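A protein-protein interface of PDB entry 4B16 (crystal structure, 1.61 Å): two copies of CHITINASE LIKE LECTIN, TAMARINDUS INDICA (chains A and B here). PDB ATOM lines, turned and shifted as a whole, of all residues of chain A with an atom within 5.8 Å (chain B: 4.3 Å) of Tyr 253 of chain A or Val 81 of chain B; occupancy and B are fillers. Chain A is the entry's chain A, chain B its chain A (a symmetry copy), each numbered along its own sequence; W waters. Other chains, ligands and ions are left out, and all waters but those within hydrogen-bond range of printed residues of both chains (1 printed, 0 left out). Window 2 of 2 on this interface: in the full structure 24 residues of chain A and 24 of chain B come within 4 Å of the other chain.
The backbone carbonyl oxygen of Gly 11 of chain A lies within hydrogen-bond range of the side-chain amide nitrogen of Gln 80 of chain B (3.0 Å). The backbone carbonyl oxygen (O) of Val 81 of chain B sits at hydrogen-bond distance from the side-chain hydroxyl (OH) of Tyr 253 of chain A (3.2 Å).
The side-chain hydroxyl of Ser 16 of chain A sits at hydrogen-bond distance from the backbone carbonyl oxygen of Gly 11 of chain A, at 2.7 Å. The side-chain carboxylate (OE2) of Glu 17 of chain A lies within hydrogen-bond range of the backbone NH (N) of Gly 11 of chain A (2.9 Å). The guanidinium group (NH1) of Arg 256 of chain A is in hydrogen-bond range of the backbone carbonyl oxygen (O) of Ser 16 of chain A (3.1 Å). The side-chain carboxylate (OD1) of Asp 251 of chain A lies within hydrogen-bond range of the backbone NH (N) of Tyr 253 of chain A, 3.1 Å away. The backbone carbonyl oxygen (O) of Gln 80 of chain B lies within hydrogen-bond range of the backbone NH (N) of Thr 39 of chain B (2.9 Å). The backbone carbonyl oxygen of Thr 39 of chain B sits at hydrogen-bond distance from the backbone NH of Thr 82 of chain B (2.8 Å).
Among the printed residues, merely in contact across the chains: Tyr 253 of chain A with Gln 80 of chain B (3.3 Å), Phe 257 of chain A with Thr 82 of chain B (3.4 Å), Tyr 253 of chain A with Thr 82 of chain B (3.4 Å), Tyr 253 of chain A with Pro 83 of chain B (3.5 Å), Phe 257 of chain A with Pro 83 of chain B (3.5 Å), Ser 16 of chain A with Thr 82 of chain B (3.6 Å) and Ser 16 of chain A with Gln 80 of chain B (3.9 Å).
Printed residues of chain B within 4 Å of Tyr 253 of chain A: Gln 80 (3.3 Å), Val 81 (3.2 Å), Thr 82 (3.4 Å) and Pro 83 (3.5 Å). Thr 39 of chain B touches none of the printed residues of chain A. Of the printed residues of chain A, Gln 80 of chain B touches Gly 11 (3.0 Å), Ser 16 (3.9 Å) and Tyr 253 (3.3 Å). Val 81 of chain B touches just one residue of chain A: Tyr 253. Of the printed residues of chain A, Thr 82 of chain B touches Ser 16 (3.6 Å), Tyr 253 (3.4 Å) and Phe 257 (3.4 Å). The nearest printed residue of chain B that does not touch Ser 16 of chain A is Pro 83 of chain B (6.7 Å).
Of the 10 printed residues of chain B, 4 touch a printed residue of chain A. Hydrophobic or aromatic side chains of chain B that line the printed part of chain A: Pro 83. Hydrophobic or aromatic side chains of chain A within 4 Å of the printed part of chain B: Tyr 253 and Phe 257. Among the printed residues, 9 pairs touch across the chains. Among the printed residues, no Asp or Glu carboxylate lies within 4 Å of a Lys or Arg side-chain nitrogen of the other chain.
No position is printed for both chains. Of the 9 pairs that touch across the chains among the printed residues, none has its exchanged pair printed and touching as well.
Water W1 lies within hydrogen-bond range of OH of Tyr 253 of chain A (2.7 Å) and O of Val 81 of chain B (3.0 Å).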
ATOM      1  N   TYR A   7      -4.777  12.351 -13.225  1.00  0.00           N
ATOM      2  CA  TYR A   7      -5.216  13.057 -12.021  1.00  0.00           C
ATOM      3  C   TYR A   7      -5.729  14.452 -12.396  1.00  0.00           C
ATOM      4  O   TYR A   7      -5.093  15.165 -13.181  1.00  0.00           O
ATOM      5  CB  TYR A   7      -4.054  13.236 -11.042  1.00  0.00           C
ATOM      6  CG  TYR A   7      -3.490  11.968 -10.447  1.00  0.00           C
ATOM      7  CD1 TYR A   7      -4.158  11.294  -9.420  1.00  0.00           C
ATOM      8  CD2 TYR A   7      -2.262  11.453 -10.883  1.00  0.00           C
ATOM      9  CE1 TYR A   7      -3.628  10.138  -8.854  1.00  0.00           C
ATOM     10  CE2 TYR A   7      -1.724  10.308 -10.318  1.00  0.00           C
ATOM     11  CZ  TYR A   7      -2.407   9.646  -9.308  1.00  0.00           C
ATOM     12  OH  TYR A   7      -1.862   8.497  -8.762  1.00  0.00           O
ATOM     13  N   GLY A  11      -4.961  21.164 -10.010  1.00  0.00           N
ATOM     14  CA  GLY A  11      -4.192  21.969 -10.974  1.00  0.00           C
ATOM     15  C   GLY A  11      -4.623  23.418 -11.040  1.00  0.00           C
ATOM     16  O   GLY A  11      -4.224  24.142 -11.959  1.00  0.00           O
ATOM     17  N   SER A  16      -6.935  27.362 -15.374  1.00  0.00           N
ATOM     18  CA  SER A  16      -5.563  26.847 -15.372  1.00  0.00           C
ATOM     19  C   SER A  16      -5.474  25.412 -15.857  1.00  0.00           C
ATOM     20  O   SER A  16      -4.639  25.108 -16.704  1.00  0.00           O
ATOM     21  CB  SER A  16      -4.871  27.029 -14.010  1.00  0.00           C
ATOM     22  OG  SER A  16      -5.516  26.280 -12.995  1.00  0.00           O
ATOM     23  N   GLU A  17      -6.329  24.527 -15.347  1.00  0.00           N
ATOM     24  CA  GLU A  17      -6.228  23.133 -15.767  1.00  0.00           C
ATOM     25  C   GLU A  17      -7.421  22.597 -16.560  1.00  0.00           C
ATOM     26  O   GLU A  17      -7.434  21.425 -16.909  1.00  0.00           O
ATOM     27  CB  GLU A  17      -5.853  22.207 -14.605  1.00  0.00           C
ATOM     28  CG  GLU A  17      -6.991  21.812 -13.713  1.00  0.00           C
ATOM     29  CD  GLU A  17      -6.671  20.624 -12.790  1.00  0.00           C
ATOM     30  OE1 GLU A  17      -5.885  19.706 -13.135  1.00  0.00           O
ATOM     31  OE2 GLU A  17      -7.217  20.618 -11.691  1.00  0.00           O
ATOM     32  N   ASP A 251      -0.048  15.478 -14.426  1.00  0.00           N
ATOM     33  CA  ASP A 251      -1.474  15.438 -14.077  1.00  0.00           C
ATOM     34  C   ASP A 251      -2.198  16.178 -15.217  1.00  0.00           C
ATOM     35  O   ASP A 251      -1.566  16.530 -16.233  1.00  0.00           O
ATOM     36  CB  ASP A 251      -1.711  16.125 -12.724  1.00  0.00           C
ATOM     37  CG  ASP A 251      -1.011  17.483 -12.628  1.00  0.00           C
ATOM     38  OD1 ASP A 251      -0.938  18.186 -13.663  1.00  0.00           O
ATOM     39  OD2 ASP A 251      -0.531  17.849 -11.525  1.00  0.00           O
ATOM     40  N   ARG A 252      -3.496  16.443 -15.073  1.00  0.00           N
ATOM     41  CA  ARG A 252      -4.225  17.092 -16.165  1.00  0.00           C
ATOM     42  C   ARG A 252      -3.683  18.484 -16.469  1.00  0.00           C
ATOM     43  O   ARG A 252      -3.628  18.878 -17.636  1.00  0.00           O
ATOM     44  CB  ARG A 252      -5.736  17.127 -15.896  1.00  0.00           C
ATOM     45  CG  ARG A 252      -6.564  17.877 -16.932  1.00  0.00           C
ATOM     46  CD  ARG A 252      -6.433  17.321 -18.354  1.00  0.00           C
ATOM     47  NE  ARG A 252      -7.201  18.160 -19.274  1.00  0.00           N
ATOM     48  CZ  ARG A 252      -7.031  18.191 -20.592  1.00  0.00           C
ATOM     49  NH1 ARG A 252      -6.169  17.367 -21.175  1.00  0.00           N
ATOM     50  NH2 ARG A 252      -7.760  19.028 -21.329  1.00  0.00           N
ATOM     51  N   TYR A 253      -3.286  19.223 -15.433  1.00  0.00           N
ATOM     52  CA  TYR A 253      -2.710  20.546 -15.648  1.00  0.00           C
ATOM     53  C   TYR A 253      -1.516  20.481 -16.624  1.00  0.00           C
ATOM     54  O   TYR A 253      -1.495  21.179 -17.652  1.00  0.00           O
ATOM     55  CB  TYR A 253      -2.320  21.219 -14.319  1.00  0.00           C
ATOM     56  CG  TYR A 253      -1.529  22.484 -14.539  1.00  0.00           C
ATOM     57  CD1 TYR A 253      -2.115  23.595 -15.162  1.00  0.00           C
ATOM     58  CD2 TYR A 253      -0.188  22.564 -14.161  1.00  0.00           C
ATOM     59  CE1 TYR A 253      -1.382  24.747 -15.403  1.00  0.00           C
ATOM     60  CE2 TYR A 253       0.558  23.723 -14.383  1.00  0.00           C
ATOM     61  CZ  TYR A 253      -0.048  24.806 -15.011  1.00  0.00           C
ATOM     62  OH  TYR A 253       0.669  25.960 -15.229  1.00  0.00           O
ATOM     63  N   PHE A 254      -0.533  19.642 -16.313  1.00  0.00           N
ATOM     64  CA  PHE A 254       0.649  19.540 -17.170  1.00  0.00           C
ATOM     65  C   PHE A 254       0.286  18.982 -18.542  1.00  0.00           C
ATOM     66  O   PHE A 254       0.768  19.479 -19.562  1.00  0.00           O
ATOM     67  CB  PHE A 254       1.740  18.698 -16.504  1.00  0.00           C
ATOM     68  CG  PHE A 254       2.259  19.295 -15.230  1.00  0.00           C
ATOM     69  CD1 PHE A 254       2.735  20.599 -15.207  1.00  0.00           C
ATOM     70  CD2 PHE A 254       2.268  18.555 -14.046  1.00  0.00           C
ATOM     71  CE1 PHE A 254       3.219  21.157 -14.030  1.00  0.00           C
ATOM     72  CE2 PHE A 254       2.742  19.110 -12.866  1.00  0.00           C
ATOM     73  CZ  PHE A 254       3.218  20.411 -12.859  1.00  0.00           C
ATOM     74  N   ASP A 255      -0.583  17.970 -18.571  1.00  0.00           N
ATOM     75  CA  ASP A 255      -0.935  17.315 -19.835  1.00  0.00           C
ATOM     76  C   ASP A 255      -1.724  18.230 -20.777  1.00  0.00           C
ATOM     77  O   ASP A 255      -1.610  18.123 -22.003  1.00  0.00           O
ATOM     78  CB  ASP A 255      -1.721  16.032 -19.556  1.00  0.00           C
ATOM     79  CG  ASP A 255      -1.617  15.018 -20.676  1.00  0.00           C
ATOM     80  OD1 ASP A 255      -0.536  14.915 -21.303  1.00  0.00           O
ATOM     81  OD2 ASP A 255      -2.610  14.279 -20.894  1.00  0.00           O
ATOM     82  N   ARG A 256      -2.534  19.114 -20.202  1.00  0.00           N
ATOM     83  CA  ARG A 256      -3.335  20.053 -20.987  1.00  0.00           C
ATOM     84  C   ARG A 256      -2.446  20.896 -21.912  1.00  0.00           C
ATOM     85  O   ARG A 256      -2.809  21.172 -23.061  1.00  0.00           O
ATOM     86  CB  ARG A 256      -4.108  20.962 -20.035  1.00  0.00           C
ATOM     87  CG  ARG A 256      -5.100  21.888 -20.702  1.00  0.00           C
ATOM     88  CD  ARG A 256      -5.690  22.803 -19.650  1.00  0.00           C
ATOM     89  NE  ARG A 256      -6.948  23.395 -20.085  1.00  0.00           N
ATOM     90  CZ  ARG A 256      -7.304  24.658 -19.860  1.00  0.00           C
ATOM     91  NH1 ARG A 256      -6.495  25.492 -19.209  1.00  0.00           N
ATOM     92  NH2 ARG A 256      -8.482  25.082 -20.283  1.00  0.00           N
ATOM     93  N   PHE A 257      -1.282  21.287 -21.399  1.00  0.00           N
ATOM     94  CA  PHE A 257      -0.345  22.132 -22.134  1.00  0.00           C
ATOM     95  C   PHE A 257       0.721  21.355 -22.883  1.00  0.00           C
ATOM     96  O   PHE A 257       1.094  21.746 -23.980  1.00  0.00           O
ATOM     97  CB  PHE A 257       0.266  23.183 -21.200  1.00  0.00           C
ATOM     98  CG  PHE A 257      -0.752  24.146 -20.693  1.00  0.00           C
ATOM     99  CD1 PHE A 257      -1.190  25.195 -21.499  1.00  0.00           C
ATOM    100  CD2 PHE A 257      -1.345  23.960 -19.438  1.00  0.00           C
ATOM    101  CE1 PHE A 257      -2.175  26.065 -21.056  1.00  0.00           C
ATOM    102  CE2 PHE A 257      -2.327  24.832 -18.987  1.00  0.00           C
ATOM    103  CZ  PHE A 257      -2.750  25.876 -19.803  1.00  0.00           C
ATOM    104  N   ARG A 258       1.181  20.247 -22.304  1.00  0.00           N
ATOM    105  CA  ARG A 258       2.298  19.484 -22.872  1.00  0.00           C
ATOM    106  C   ARG A 258       1.845  18.449 -23.899  1.00  0.00           C
ATOM    107  O   ARG A 258       2.646  18.017 -24.744  1.00  0.00           O
ATOM    108  CB  ARG A 258       3.081  18.765 -21.766  1.00  0.00           C
ATOM    109  CG  ARG A 258       3.673  19.657 -20.683  1.00  0.00           C
ATOM    110  CD  ARG A 258       5.003  20.236 -21.093  1.00  0.00           C
ATOM    111  NE  ARG A 258       5.454  21.260 -20.156  1.00  0.00           N
ATOM    112  CZ  ARG A 258       6.600  21.920 -20.283  1.00  0.00           C
ATOM    113  NH1 ARG A 258       7.406  21.650 -21.302  1.00  0.00           N
ATOM    114  NH2 ARG A 258       6.938  22.853 -19.399  1.00  0.00           N
ATOM    115  N   THR B  39      -1.007  32.732 -11.692  1.00  0.00           N
ATOM    116  CA  THR B  39      -0.884  33.813 -12.671  1.00  0.00           C
ATOM    117  C   THR B  39      -0.796  33.267 -14.091  1.00  0.00           C
ATOM    118  O   THR B  39      -0.442  32.092 -14.294  1.00  0.00           O
ATOM    119  CB  THR B  39       0.296  34.775 -12.336  1.00  0.00           C
ATOM    120  OG1 THR B  39       1.567  34.088 -12.476  1.00  0.00           O
ATOM    121  CG2 THR B  39       0.121  35.340 -10.908  1.00  0.00           C
ATOM    122  N   GLN B  80       2.199  29.386  -9.318  1.00  0.00           N
ATOM    123  CA  GLN B  80       1.885  28.699 -10.560  1.00  0.00           C
ATOM    124  C   GLN B  80       1.787  29.734 -11.661  1.00  0.00           C
ATOM    125  O   GLN B  80       1.062  30.719 -11.512  1.00  0.00           O
ATOM    126  CB  GLN B  80       0.542  27.955 -10.385  1.00  0.00           C
ATOM    127  CG  GLN B  80       0.076  27.140 -11.587  1.00  0.00           C
ATOM    128  CD  GLN B  80      -1.202  26.372 -11.299  1.00  0.00           C
ATOM    129  OE1 GLN B  80      -1.754  26.458 -10.204  1.00  0.00           O
ATOM    130  NE2 GLN B  80      -1.667  25.601 -12.271  1.00  0.00           N
ATOM    131  N   VAL B  81       2.535  29.521 -12.750  1.00  0.00           N
ATOM    132  CA  VAL B  81       2.446  30.358 -13.944  1.00  0.00           C
ATOM    133  C   VAL B  81       1.914  29.494 -15.074  1.00  0.00           C
ATOM    134  O   VAL B  81       2.587  28.549 -15.514  1.00  0.00           O
ATOM    135  CB  VAL B  81       3.816  30.961 -14.348  1.00  0.00           C
ATOM    136  CG1 VAL B  81       3.666  31.818 -15.602  1.00  0.00           C
ATOM    137  CG2 VAL B  81       4.368  31.812 -13.209  1.00  0.00           C
ATOM    138  N   THR B  82       0.702  29.812 -15.525  1.00  0.00           N
ATOM    139  CA  THR B  82       0.035  29.034 -16.562  1.00  0.00           C
ATOM    140  C   THR B  82       0.614  29.491 -17.912  1.00  0.00           C
ATOM    141  O   THR B  82       0.439  30.639 -18.299  1.00  0.00           O
ATOM    142  CB  THR B  82      -1.499  29.238 -16.512  1.00  0.00           C
ATOM    143  OG1 THR B  82      -2.013  28.865 -15.210  1.00  0.00           O
ATOM    144  CG2 THR B  82      -2.186  28.394 -17.578  1.00  0.00           C
ATOM    145  N   PRO B  83       1.339  28.603 -18.618  1.00  0.00           N
ATOM    146  CA  PRO B  83       2.102  29.054 -19.786  1.00  0.00           C
ATOM    147  C   PRO B  83       1.238  29.294 -21.022  1.00  0.00           C
ATOM    148  O   PRO B  83       0.117  28.775 -21.122  1.00  0.00           O
ATOM    149  CB  PRO B  83       3.073  27.892 -20.024  1.00  0.00           C
ATOM    150  CG  PRO B  83       2.294  26.700 -19.576  1.00  0.00           C
ATOM    151  CD  PRO B  83       1.526  27.163 -18.366  1.00  0.00           C
ATOM    152  N   PRO B 125       8.435  27.151 -12.859  1.00  0.00           N
ATOM    153  CA  PRO B 125       8.744  27.802 -14.140  1.00  0.00           C
ATOM    154  C   PRO B 125       8.025  29.139 -14.289  1.00  0.00           C
ATOM    155  O   PRO B 125       6.869  29.285 -13.883  1.00  0.00           O
ATOM    156  CB  PRO B 125       8.230  26.808 -15.199  1.00  0.00           C
ATOM    157  CG  PRO B 125       7.942  25.540 -14.487  1.00  0.00           C
ATOM    158  CD  PRO B 125       7.850  25.803 -13.018  1.00  0.00           C
ATOM    159  N   GLU B 126       8.712  30.111 -14.869  1.00  0.00           N
ATOM    160  CA  GLU B 126       8.070  31.358 -15.248  1.00  0.00           C
ATOM    161  C   GLU B 126       7.418  31.163 -16.629  1.00  0.00           C
ATOM    162  O   GLU B 126       7.219  30.034 -17.074  1.00  0.00           O
ATOM    163  CB  GLU B 126       9.080  32.524 -15.196  1.00  0.00           C
ATOM    164  CG  GLU B 126      10.203  32.438 -16.229  1.00  0.00           C
ATOM    165  CD  GLU B 126      11.335  33.406 -15.955  1.00  0.00           C
ATOM    166  OE1 GLU B 126      11.227  34.213 -15.010  1.00  0.00           O
ATOM    167  OE2 GLU B 126      12.353  33.347 -16.676  1.00  0.00           O
ATOM    168  N   GLY B 127       7.059  32.243 -17.295  1.00  0.00           N
ATOM    169  CA  GLY B 127       6.393  32.127 -18.590  1.00  0.00           C
ATOM    170  C   GLY B 127       7.301  32.461 -19.758  1.00  0.00           C
ATOM    171  O   GLY B 127       8.488  32.759 -19.584  1.00  0.00           O
ATOM    172  N   LEU B 130       5.732  36.250 -19.003  1.00  0.00           N
ATOM    173  CA  LEU B 130       5.922  36.667 -17.603  1.00  0.00           C
ATOM    174  C   LEU B 130       7.300  36.239 -17.098  1.00  0.00           C
ATOM    175  O   LEU B 130       7.622  35.056 -17.128  1.00  0.00           O
ATOM    176  CB  LEU B 130       4.827  36.072 -16.696  1.00  0.00           C
ATOM    177  CG  LEU B 130       5.006  36.391 -15.198  1.00  0.00           C
ATOM    178  CD1 LEU B 130       4.914  37.899 -14.930  1.00  0.00           C
ATOM    179  CD2 LEU B 130       4.033  35.615 -14.319  1.00  0.00           C
ATOM    180  N   PHE B 132      10.063  36.503 -13.814  1.00  0.00           N
ATOM    181  CA  PHE B 132      10.129  36.788 -12.379  1.00  0.00           C
ATOM    182  C   PHE B 132      11.095  37.922 -11.998  1.00  0.00           C
ATOM    183  O   PHE B 132      10.763  38.752 -11.151  1.00  0.00           O
ATOM    184  CB  PHE B 132      10.506  35.538 -11.589  1.00  0.00           C
ATOM    185  CG  PHE B 132       9.470  34.439 -11.611  1.00  0.00           C
ATOM    186  CD1 PHE B 132       8.103  34.715 -11.726  1.00  0.00           C
ATOM    187  CD2 PHE B 132       9.875  33.112 -11.448  1.00  0.00           C
ATOM    188  CE1 PHE B 132       7.167  33.682 -11.705  1.00  0.00           C
ATOM    189  CE2 PHE B 132       8.943  32.079 -11.411  1.00  0.00           C
ATOM    190  CZ  PHE B 132       7.589  32.365 -11.544  1.00  0.00           C
HETATM  191  O   HOH W   1       3.317  25.716 -14.741  1.00  0.00           O
